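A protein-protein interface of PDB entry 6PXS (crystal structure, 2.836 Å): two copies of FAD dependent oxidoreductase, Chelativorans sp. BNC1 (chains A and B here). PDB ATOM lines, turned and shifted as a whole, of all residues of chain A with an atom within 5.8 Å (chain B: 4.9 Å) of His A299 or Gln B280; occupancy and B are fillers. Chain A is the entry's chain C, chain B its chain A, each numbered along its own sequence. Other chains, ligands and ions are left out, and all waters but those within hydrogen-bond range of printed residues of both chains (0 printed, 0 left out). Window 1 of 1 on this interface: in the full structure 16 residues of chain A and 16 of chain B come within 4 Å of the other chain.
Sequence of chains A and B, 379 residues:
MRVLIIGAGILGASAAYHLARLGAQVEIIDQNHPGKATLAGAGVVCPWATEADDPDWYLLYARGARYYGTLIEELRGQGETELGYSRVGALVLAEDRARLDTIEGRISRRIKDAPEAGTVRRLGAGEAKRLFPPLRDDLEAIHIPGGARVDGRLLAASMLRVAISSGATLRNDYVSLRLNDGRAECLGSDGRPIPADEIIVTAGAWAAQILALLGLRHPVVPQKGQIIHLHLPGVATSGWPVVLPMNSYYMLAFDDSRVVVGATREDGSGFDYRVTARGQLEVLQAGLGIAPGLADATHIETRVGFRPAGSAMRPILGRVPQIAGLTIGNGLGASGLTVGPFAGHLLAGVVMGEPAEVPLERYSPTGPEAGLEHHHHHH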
ATOM      1  N   ILE A 228     -12.477  11.057   6.509  1.00  0.00           N
ATOM      2  CA  ILE A 228     -12.156  10.214   5.362  1.00  0.00           C
ATOM      3  C   ILE A 228     -11.391  11.027   4.329  1.00  0.00           C
ATOM      4  O   ILE A 228     -11.748  12.174   4.032  1.00  0.00           O
ATOM      5  CB  ILE A 228     -13.428   9.611   4.736  1.00  0.00           C
ATOM      6  CG1 ILE A 228     -14.056   8.597   5.691  1.00  0.00           C
ATOM      7  CG2 ILE A 228     -13.100   8.969   3.392  1.00  0.00           C
ATOM      8  CD1 ILE A 228     -15.406   8.092   5.244  1.00  0.00           C
ATOM      9  N   HIS A 229     -10.348  10.418   3.769  1.00  0.00           N
ATOM     10  CA  HIS A 229      -9.554  11.006   2.698  1.00  0.00           C
ATOM     11  C   HIS A 229      -9.799  10.227   1.413  1.00  0.00           C
ATOM     12  O   HIS A 229      -9.759   8.992   1.417  1.00  0.00           O
ATOM     13  CB  HIS A 229      -8.064  10.989   3.048  1.00  0.00           C
ATOM     14  CG  HIS A 229      -7.695  11.908   4.170  1.00  0.00           C
ATOM     15  ND1 HIS A 229      -6.773  12.922   4.027  1.00  0.00           N
ATOM     16  CD2 HIS A 229      -8.123  11.967   5.453  1.00  0.00           C
ATOM     17  CE1 HIS A 229      -6.649  13.566   5.174  1.00  0.00           C
ATOM     18  NE2 HIS A 229      -7.457  13.006   6.056  1.00  0.00           N
ATOM     19  N   LEU A 230     -10.050  10.945   0.322  1.00  0.00           N
ATOM     20  CA  LEU A 230     -10.330  10.341  -0.970  1.00  0.00           C
ATOM     21  C   LEU A 230      -9.320  10.824  -2.002  1.00  0.00           C
ATOM     22  O   LEU A 230      -8.632  11.828  -1.806  1.00  0.00           O
ATOM     23  CB  LEU A 230     -11.753  10.670  -1.438  1.00  0.00           C
ATOM     24  CG  LEU A 230     -12.881  10.247  -0.496  1.00  0.00           C
ATOM     25  CD1 LEU A 230     -14.229  10.657  -1.061  1.00  0.00           C
ATOM     26  CD2 LEU A 230     -12.844   8.748  -0.243  1.00  0.00           C
ATOM     27  N   HIS A 231      -9.246  10.096  -3.114  1.00  0.00           N
ATOM     28  CA  HIS A 231      -8.292  10.390  -4.178  1.00  0.00           C
ATOM     29  C   HIS A 231      -8.991  10.259  -5.522  1.00  0.00           C
ATOM     30  O   HIS A 231      -9.580   9.214  -5.816  1.00  0.00           O
ATOM     31  CB  HIS A 231      -7.086   9.446  -4.102  1.00  0.00           C
ATOM     32  CG  HIS A 231      -6.103   9.623  -5.216  1.00  0.00           C
ATOM     33  ND1 HIS A 231      -5.329  10.756  -5.353  1.00  0.00           N
ATOM     34  CD2 HIS A 231      -5.764   8.809  -6.244  1.00  0.00           C
ATOM     35  CE1 HIS A 231      -4.556  10.632  -6.419  1.00  0.00           C
ATOM     36  NE2 HIS A 231      -4.802   9.460  -6.977  1.00  0.00           N
ATOM     37  N   GLN A 280     -17.882   5.675   9.492  1.00  0.00           N
ATOM     38  CA  GLN A 280     -17.560   5.871   8.085  1.00  0.00           C
ATOM     39  C   GLN A 280     -18.804   5.846   7.209  1.00  0.00           C
ATOM     40  O   GLN A 280     -18.815   6.464   6.139  1.00  0.00           O
ATOM     41  CB  GLN A 280     -16.566   4.808   7.623  1.00  0.00           C
ATOM     42  CG  GLN A 280     -15.191   4.978   8.239  1.00  0.00           C
ATOM     43  CD  GLN A 280     -14.148   4.114   7.576  1.00  0.00           C
ATOM     44  OE1 GLN A 280     -13.211   4.615   6.955  1.00  0.00           O
ATOM     45  NE2 GLN A 280     -14.299   2.806   7.707  1.00  0.00           N
ATOM     46  N   LEU A 284     -19.697   8.932   4.621  1.00  0.00           N
ATOM     47  CA  LEU A 284     -19.858   8.634   3.201  1.00  0.00           C
ATOM     48  C   LEU A 284     -21.253   9.002   2.710  1.00  0.00           C
ATOM     49  O   LEU A 284     -21.413   9.476   1.580  1.00  0.00           O
ATOM     50  CB  LEU A 284     -19.566   7.157   2.942  1.00  0.00           C
ATOM     51  CG  LEU A 284     -18.106   6.734   3.117  1.00  0.00           C
ATOM     52  CD1 LEU A 284     -17.990   5.219   3.126  1.00  0.00           C
ATOM     53  CD2 LEU A 284     -17.237   7.329   2.020  1.00  0.00           C
ATOM     54  N   ALA A 297     -14.354   7.382  -6.357  1.00  0.00           N
ATOM     55  CA  ALA A 297     -13.061   7.873  -5.908  1.00  0.00           C
ATOM     56  C   ALA A 297     -12.406   6.860  -4.978  1.00  0.00           C
ATOM     57  O   ALA A 297     -13.078   6.160  -4.218  1.00  0.00           O
ATOM     58  CB  ALA A 297     -13.210   9.215  -5.191  1.00  0.00           C
ATOM     59  N   THR A 298     -11.080   6.791  -5.044  1.00  0.00           N
ATOM     60  CA  THR A 298     -10.342   5.866  -4.197  1.00  0.00           C
ATOM     61  C   THR A 298     -10.392   6.317  -2.744  1.00  0.00           C
ATOM     62  O   THR A 298     -10.210   7.498  -2.436  1.00  0.00           O
ATOM     63  CB  THR A 298      -8.884   5.769  -4.644  1.00  0.00           C
ATOM     64  OG1 THR A 298      -8.822   5.478  -6.045  1.00  0.00           O
ATOM     65  CG2 THR A 298      -8.164   4.678  -3.867  1.00  0.00           C
ATOM     66  N   HIS A 299     -10.642   5.367  -1.847  1.00  0.00           N
ATOM     67  CA  HIS A 299     -10.522   5.602  -0.414  1.00  0.00           C
ATOM     68  C   HIS A 299      -9.117   5.185   0.005  1.00  0.00           C
ATOM     69  O   HIS A 299      -8.774   4.001  -0.052  1.00  0.00           O
ATOM     70  CB  HIS A 299     -11.584   4.824   0.358  1.00  0.00           C
ATOM     71  CG  HIS A 299     -11.647   5.171   1.814  1.00  0.00           C
ATOM     72  ND1 HIS A 299     -12.646   4.715   2.644  1.00  0.00           N
ATOM     73  CD2 HIS A 299     -10.838   5.936   2.585  1.00  0.00           C
ATOM     74  CE1 HIS A 299     -12.449   5.179   3.865  1.00  0.00           C
ATOM     75  NE2 HIS A 299     -11.358   5.923   3.855  1.00  0.00           N
ATOM     76  N   ILE A 300      -8.303   6.153   0.417  1.00  0.00           N
ATOM     77  CA  ILE A 300      -6.909   5.897   0.755  1.00  0.00           C
ATOM     78  C   ILE A 300      -6.719   5.687   2.252  1.00  0.00           C
ATOM     79  O   ILE A 300      -5.994   4.782   2.663  1.00  0.00           O
ATOM     80  CB  ILE A 300      -5.995   7.026   0.230  1.00  0.00           C
ATOM     81  CG1 ILE A 300      -6.511   8.405   0.645  1.00  0.00           C
ATOM     82  CG2 ILE A 300      -5.872   6.939  -1.286  1.00  0.00           C
ATOM     83  CD1 ILE A 300      -5.607   9.545   0.208  1.00  0.00           C
ATOM     84  N   GLU A 301      -7.359   6.500   3.089  1.00  0.00           N
ATOM     85  CA  GLU A 301      -7.253   6.293   4.526  1.00  0.00           C
ATOM     86  C   GLU A 301      -8.394   7.005   5.231  1.00  0.00           C
ATOM     87  O   GLU A 301      -9.051   7.885   4.668  1.00  0.00           O
ATOM     88  CB  GLU A 301      -5.907   6.785   5.074  1.00  0.00           C
ATOM     89  CG  GLU A 301      -5.663   8.281   4.915  1.00  0.00           C
ATOM     90  CD  GLU A 301      -4.514   8.781   5.773  1.00  0.00           C
ATOM     91  OE1 GLU A 301      -4.263   8.189   6.845  1.00  0.00           O
ATOM     92  OE2 GLU A 301      -3.862   9.772   5.378  1.00  0.00           O
ATOM     93  N   THR A 302      -8.617   6.601   6.479  1.00  0.00           N
ATOM     94  CA  THR A 302      -9.531   7.278   7.389  1.00  0.00           C
ATOM     95  C   THR A 302      -8.781   7.534   8.684  1.00  0.00           C
ATOM     96  O   THR A 302      -8.238   6.599   9.281  1.00  0.00           O
ATOM     97  CB  THR A 302     -10.786   6.441   7.644  1.00  0.00           C
ATOM     98  OG1 THR A 302     -11.506   6.273   6.417  1.00  0.00           O
ATOM     99  CG2 THR A 302     -11.688   7.116   8.669  1.00  0.00           C
ATOM    100  N   GLN B 226     -15.961  -5.439  -3.866  1.00  0.00           N
ATOM    101  CA  GLN B 226     -15.365  -4.923  -2.641  1.00  0.00           C
ATOM    102  C   GLN B 226     -16.043  -5.578  -1.445  1.00  0.00           C
ATOM    103  O   GLN B 226     -17.275  -5.636  -1.381  1.00  0.00           O
ATOM    104  CB  GLN B 226     -15.503  -3.401  -2.567  1.00  0.00           C
ATOM    105  CG  GLN B 226     -15.021  -2.682  -3.815  1.00  0.00           C
ATOM    106  CD  GLN B 226     -15.103  -1.175  -3.692  1.00  0.00           C
ATOM    107  OE1 GLN B 226     -14.886  -0.613  -2.618  1.00  0.00           O
ATOM    108  NE2 GLN B 226     -15.423  -0.509  -4.795  1.00  0.00           N
ATOM    109  N   ILE B 228     -15.878  -6.029   2.944  1.00  0.00           N
ATOM    110  CA  ILE B 228     -15.427  -5.364   4.162  1.00  0.00           C
ATOM    111  C   ILE B 228     -15.200  -6.399   5.253  1.00  0.00           C
ATOM    112  O   ILE B 228     -15.975  -7.352   5.397  1.00  0.00           O
ATOM    113  CB  ILE B 228     -16.445  -4.300   4.619  1.00  0.00           C
ATOM    114  CG1 ILE B 228     -16.497  -3.156   3.604  1.00  0.00           C
ATOM    115  CG2 ILE B 228     -16.084  -3.783   6.006  1.00  0.00           C
ATOM    116  CD1 ILE B 228     -17.562  -2.129   3.889  1.00  0.00           C
ATOM    117  N   VAL B 275     -10.246   0.743  -3.963  1.00  0.00           N
ATOM    118  CA  VAL B 275     -11.321   0.736  -2.979  1.00  0.00           C
ATOM    119  C   VAL B 275     -12.068   2.055  -3.120  1.00  0.00           C
ATOM    120  O   VAL B 275     -11.543   3.116  -2.766  1.00  0.00           O
ATOM    121  CB  VAL B 275     -10.786   0.544  -1.555  1.00  0.00           C
ATOM    122  CG1 VAL B 275     -11.894   0.758  -0.535  1.00  0.00           C
ATOM    123  CG2 VAL B 275     -10.178  -0.839  -1.407  1.00  0.00           C
ATOM    124  N   THR B 276     -13.291   1.997  -3.637  1.00  0.00           N
ATOM    125  CA  THR B 276     -14.040   3.205  -3.937  1.00  0.00           C
ATOM    126  C   THR B 276     -14.930   3.603  -2.761  1.00  0.00           C
ATOM    127  O   THR B 276     -15.146   2.840  -1.817  1.00  0.00           O
ATOM    128  CB  THR B 276     -14.881   3.019  -5.201  1.00  0.00           C
ATOM    129  OG1 THR B 276     -15.898   2.039  -4.967  1.00  0.00           O
ATOM    130  CG2 THR B 276     -14.004   2.576  -6.363  1.00  0.00           C
ATOM    131  N   ALA B 277     -15.454   4.828  -2.834  1.00  0.00           N
ATOM    132  CA  ALA B 277     -16.277   5.356  -1.754  1.00  0.00           C
ATOM    133  C   ALA B 277     -17.682   4.768  -1.786  1.00  0.00           C
ATOM    134  O   ALA B 277     -18.177   4.271  -0.768  1.00  0.00           O
ATOM    135  CB  ALA B 277     -16.334   6.881  -1.841  1.00  0.00           C
ATOM    136  N   ARG B 278     -18.341   4.817  -2.945  1.00  0.00           N
ATOM    137  CA  ARG B 278     -19.704   4.304  -3.036  1.00  0.00           C
ATOM    138  C   ARG B 278     -19.743   2.799  -2.805  1.00  0.00           C
ATOM    139  O   ARG B 278     -20.654   2.292  -2.140  1.00  0.00           O
ATOM    140  CB  ARG B 278     -20.309   4.658  -4.396  1.00  0.00           C
ATOM    141  CG  ARG B 278     -21.666   4.012  -4.666  1.00  0.00           C
ATOM    142  CD  ARG B 278     -22.668   5.018  -5.214  1.00  0.00           C
ATOM    143  NE  ARG B 278     -23.282   5.810  -4.150  1.00  0.00           N
ATOM    144  CZ  ARG B 278     -24.013   6.903  -4.353  1.00  0.00           C
ATOM    145  NH1 ARG B 278     -24.223   7.352  -5.585  1.00  0.00           N
ATOM    146  NH2 ARG B 278     -24.531   7.554  -3.318  1.00  0.00           N
ATOM    147  N   GLY B 279     -18.771   2.069  -3.349  1.00  0.00           N
ATOM    148  CA  GLY B 279     -18.728   0.636  -3.115  1.00  0.00           C
ATOM    149  C   GLY B 279     -18.772   0.290  -1.641  1.00  0.00           C
ATOM    150  O   GLY B 279     -19.468  -0.642  -1.231  1.00  0.00           O
ATOM    151  N   GLN B 280     -18.042   1.047  -0.820  1.00  0.00           N
ATOM    152  CA  GLN B 280     -18.032   0.784   0.614  1.00  0.00           C
ATOM    153  C   GLN B 280     -19.312   1.267   1.284  1.00  0.00           C
ATOM    154  O   GLN B 280     -19.809   0.622   2.214  1.00  0.00           O
ATOM    155  CB  GLN B 280     -16.809   1.439   1.253  1.00  0.00           C
ATOM    156  CG  GLN B 280     -15.510   0.748   0.895  1.00  0.00           C
ATOM    157  CD  GLN B 280     -14.384   1.095   1.843  1.00  0.00           C
ATOM    158  OE1 GLN B 280     -13.963   0.270   2.653  1.00  0.00           O
ATOM    159  NE2 GLN B 280     -13.888   2.317   1.747  1.00  0.00           N
ATOM    160  N   LEU B 281     -19.860   2.395   0.827  1.00  0.00           N
ATOM    161  CA  LEU B 281     -21.122   2.876   1.380  1.00  0.00           C
ATOM    162  C   LEU B 281     -22.216   1.829   1.217  1.00  0.00           C
ATOM    163  O   LEU B 281     -22.928   1.503   2.173  1.00  0.00           O
ATOM    164  CB  LEU B 281     -21.525   4.188   0.705  1.00  0.00           C
ATOM    165  CG  LEU B 281     -22.878   4.783   1.114  1.00  0.00           C
ATOM    166  CD1 LEU B 281     -22.884   5.181   2.583  1.00  0.00           C
ATOM    167  CD2 LEU B 281     -23.231   5.979   0.245  1.00  0.00           C
ATOM    168  N   GLU B 282     -22.358   1.285   0.006  1.00  0.00           N
ATOM    169  CA  GLU B 282     -23.412   0.309  -0.247  1.00  0.00           C
ATOM    170  C   GLU B 282     -23.305  -0.878   0.700  1.00  0.00           C
ATOM    171  O   GLU B 282     -24.314  -1.342   1.244  1.00  0.00           O
ATOM    172  CB  GLU B 282     -23.352  -0.159  -1.701  1.00  0.00           C
ATOM    173  CG  GLU B 282     -23.666   0.929  -2.716  1.00  0.00           C
ATOM    174  CD  GLU B 282     -23.492   0.458  -4.146  1.00  0.00           C
ATOM    175  OE1 GLU B 282     -23.769   1.249  -5.074  1.00  0.00           O
ATOM    176  OE2 GLU B 282     -23.077  -0.706  -4.341  1.00  0.00           O
ATOM    177  N   VAL B 283     -22.087  -1.379   0.915  1.00  0.00           N
ATOM    178  CA  VAL B 283     -21.910  -2.528   1.796  1.00  0.00           C
ATOM    179  C   VAL B 283     -22.229  -2.150   3.236  1.00  0.00           C
ATOM    180  O   VAL B 283     -22.903  -2.899   3.955  1.00  0.00           O
ATOM    181  CB  VAL B 283     -20.482  -3.086   1.659  1.00  0.00           C
ATOM    182  CG1 VAL B 283     -20.263  -4.228   2.636  1.00  0.00           C
ATOM    183  CG2 VAL B 283     -20.225  -3.546   0.231  1.00  0.00           C
ATOM    184  N   LEU B 284     -21.756  -0.985   3.683  1.00  0.00           N
ATOM    185  CA  LEU B 284     -22.015  -0.566   5.058  1.00  0.00           C
ATOM    186  C   LEU B 284     -23.509  -0.406   5.315  1.00  0.00           C
ATOM    187  O   LEU B 284     -24.009  -0.801   6.375  1.00  0.00           O
ATOM    188  CB  LEU B 284     -21.272   0.736   5.356  1.00  0.00           C
ATOM    189  CG  LEU B 284     -19.745   0.633   5.438  1.00  0.00           C
ATOM    190  CD1 LEU B 284     -19.106   2.015   5.492  1.00  0.00           C
ATOM    191  CD2 LEU B 284     -19.325  -0.189   6.647  1.00  0.00           C
ATOM    192  N   HIS B 299     -13.302  -1.354  11.617  1.00  0.00           N
ATOM    193  CA  HIS B 299     -13.110  -1.653  10.203  1.00  0.00           C
ATOM    194  C   HIS B 299     -11.614  -1.837   9.978  1.00  0.00           C
ATOM    195  O   HIS B 299     -10.852  -0.866  10.004  1.00  0.00           O
ATOM    196  CB  HIS B 299     -13.676  -0.535   9.331  1.00  0.00           C
ATOM    197  CG  HIS B 299     -13.578  -0.800   7.862  1.00  0.00           C
ATOM    198  ND1 HIS B 299     -14.042   0.086   6.917  1.00  0.00           N
ATOM    199  CD2 HIS B 299     -13.072  -1.852   7.175  1.00  0.00           C
ATOM    200  CE1 HIS B 299     -13.824  -0.404   5.709  1.00  0.00           C
ATOM    201  NE2 HIS B 299     -13.237  -1.579   5.838  1.00  0.00           N
ATOM    202  N   THR B 302     -10.576  -3.561   3.675  1.00  0.00           N
ATOM    203  CA  THR B 302     -11.570  -3.762   2.624  1.00  0.00           C
ATOM    204  C   THR B 302     -10.849  -4.356   1.422  1.00  0.00           C
ATOM    205  O   THR B 302     -10.030  -3.678   0.795  1.00  0.00           O
ATOM    206  CB  THR B 302     -12.264  -2.453   2.251  1.00  0.00           C
ATOM    207  OG1 THR B 302     -12.990  -1.956   3.382  1.00  0.00           O
ATOM    208  CG2 THR B 302     -13.221  -2.663   1.084  1.00  0.00           C
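NE2 of Gln B280 sits at hydrogen-bond distance from ND1 of His A299, 2.8 Å away. A ring nitrogen (ND1) of His B299 sits at hydrogen-bond distance from the side-chain amide nitrogen (NE2) of Gln A280 (2.8 Å). The backbone NH (N) of Ala B277 lies within hydrogen-bond range of the backbone carbonyl oxygen (O) of Ala A297 (3.1 Å). The backbone NH (N) of His A299 lies within hydrogen-bond range of the backbone carbonyl oxygen (O) of Val B275, 2.6 Å away.
The side-chain hydroxyl of Thr B302 is in hydrogen-bond range of the side-chain amide oxygen of Gln B280 (2.5 Å). O of Glu A301 sits at hydrogen-bond distance from NE2 of His A299 (3.1 Å). The side-chain hydroxyl (OG1) of Thr B276 lies within hydrogen-bond range of the side-chain amide nitrogen (NE2) of Gln B226 (2.6 Å). NE2 of His A299 sits at hydrogen-bond distance from OG1 of Thr A302 (2.6 Å). The backbone NH of Gly B279 is in hydrogen-bond range of the side-chain hydroxyl of Thr B276, 3.3 Å away. The backbone carbonyl oxygen (O) of Thr A298 sits at hydrogen-bond distance from the backbone NH (N) of His A231, at 2.9 Å.
Ala B277 touches Leu A284 (CB to CD2, 3.99 Å). Leu A284 touches Leu B281. O of Ala A297 touches O of Val B275, 3.7 Å away. CA of Thr B276 touches O of Ala A297, 3.1 Å away. Thr A298 touches Val B275.
Printed residues of chain B within 4 Å of Leu A284: Ala B277 (3.99 Å) and Leu B281 (3.9 Å). Of the printed residues of chain B, Ala A297 touches Val B275, Thr B276 and Ala B277. Printed residues of chain B within 4 Å of His A299: Val B275 and Gln B280. Of the printed residues of chain A, Thr B276 touches Ala A297. Of chain A, only His A299 (2.8 Å) comes within 4 Å of Gln B280. Printed residues of chain A within 4 Å of His B299: Gln A280. The nearest residue of chain B that does not touch His A299 is Thr B276 (4.5 Å).
Hydrophobic or aromatic side chains of chain B that line the printed part of chain A: Ala B277, Leu B281 and His B299. Printed residues of chain A that touch a printed residue of chain B: Gln A280, Leu A284, Ala A297, Thr A298 and His A299. Among the printed residues, 9 pairs touch across the chains. Among the printed residues, no Asp or Glu carboxylate lies within 4 Å of a Lys or Arg side-chain nitrogen of the other chain.
Gln A280 touches His B299, and with the chains exchanged His A299 touches Gln B280. 5 positions are printed for both chains. Of the 9 pairs that touch across the chains among the printed residues, 2 have their exchanged pair printed and touching as well.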
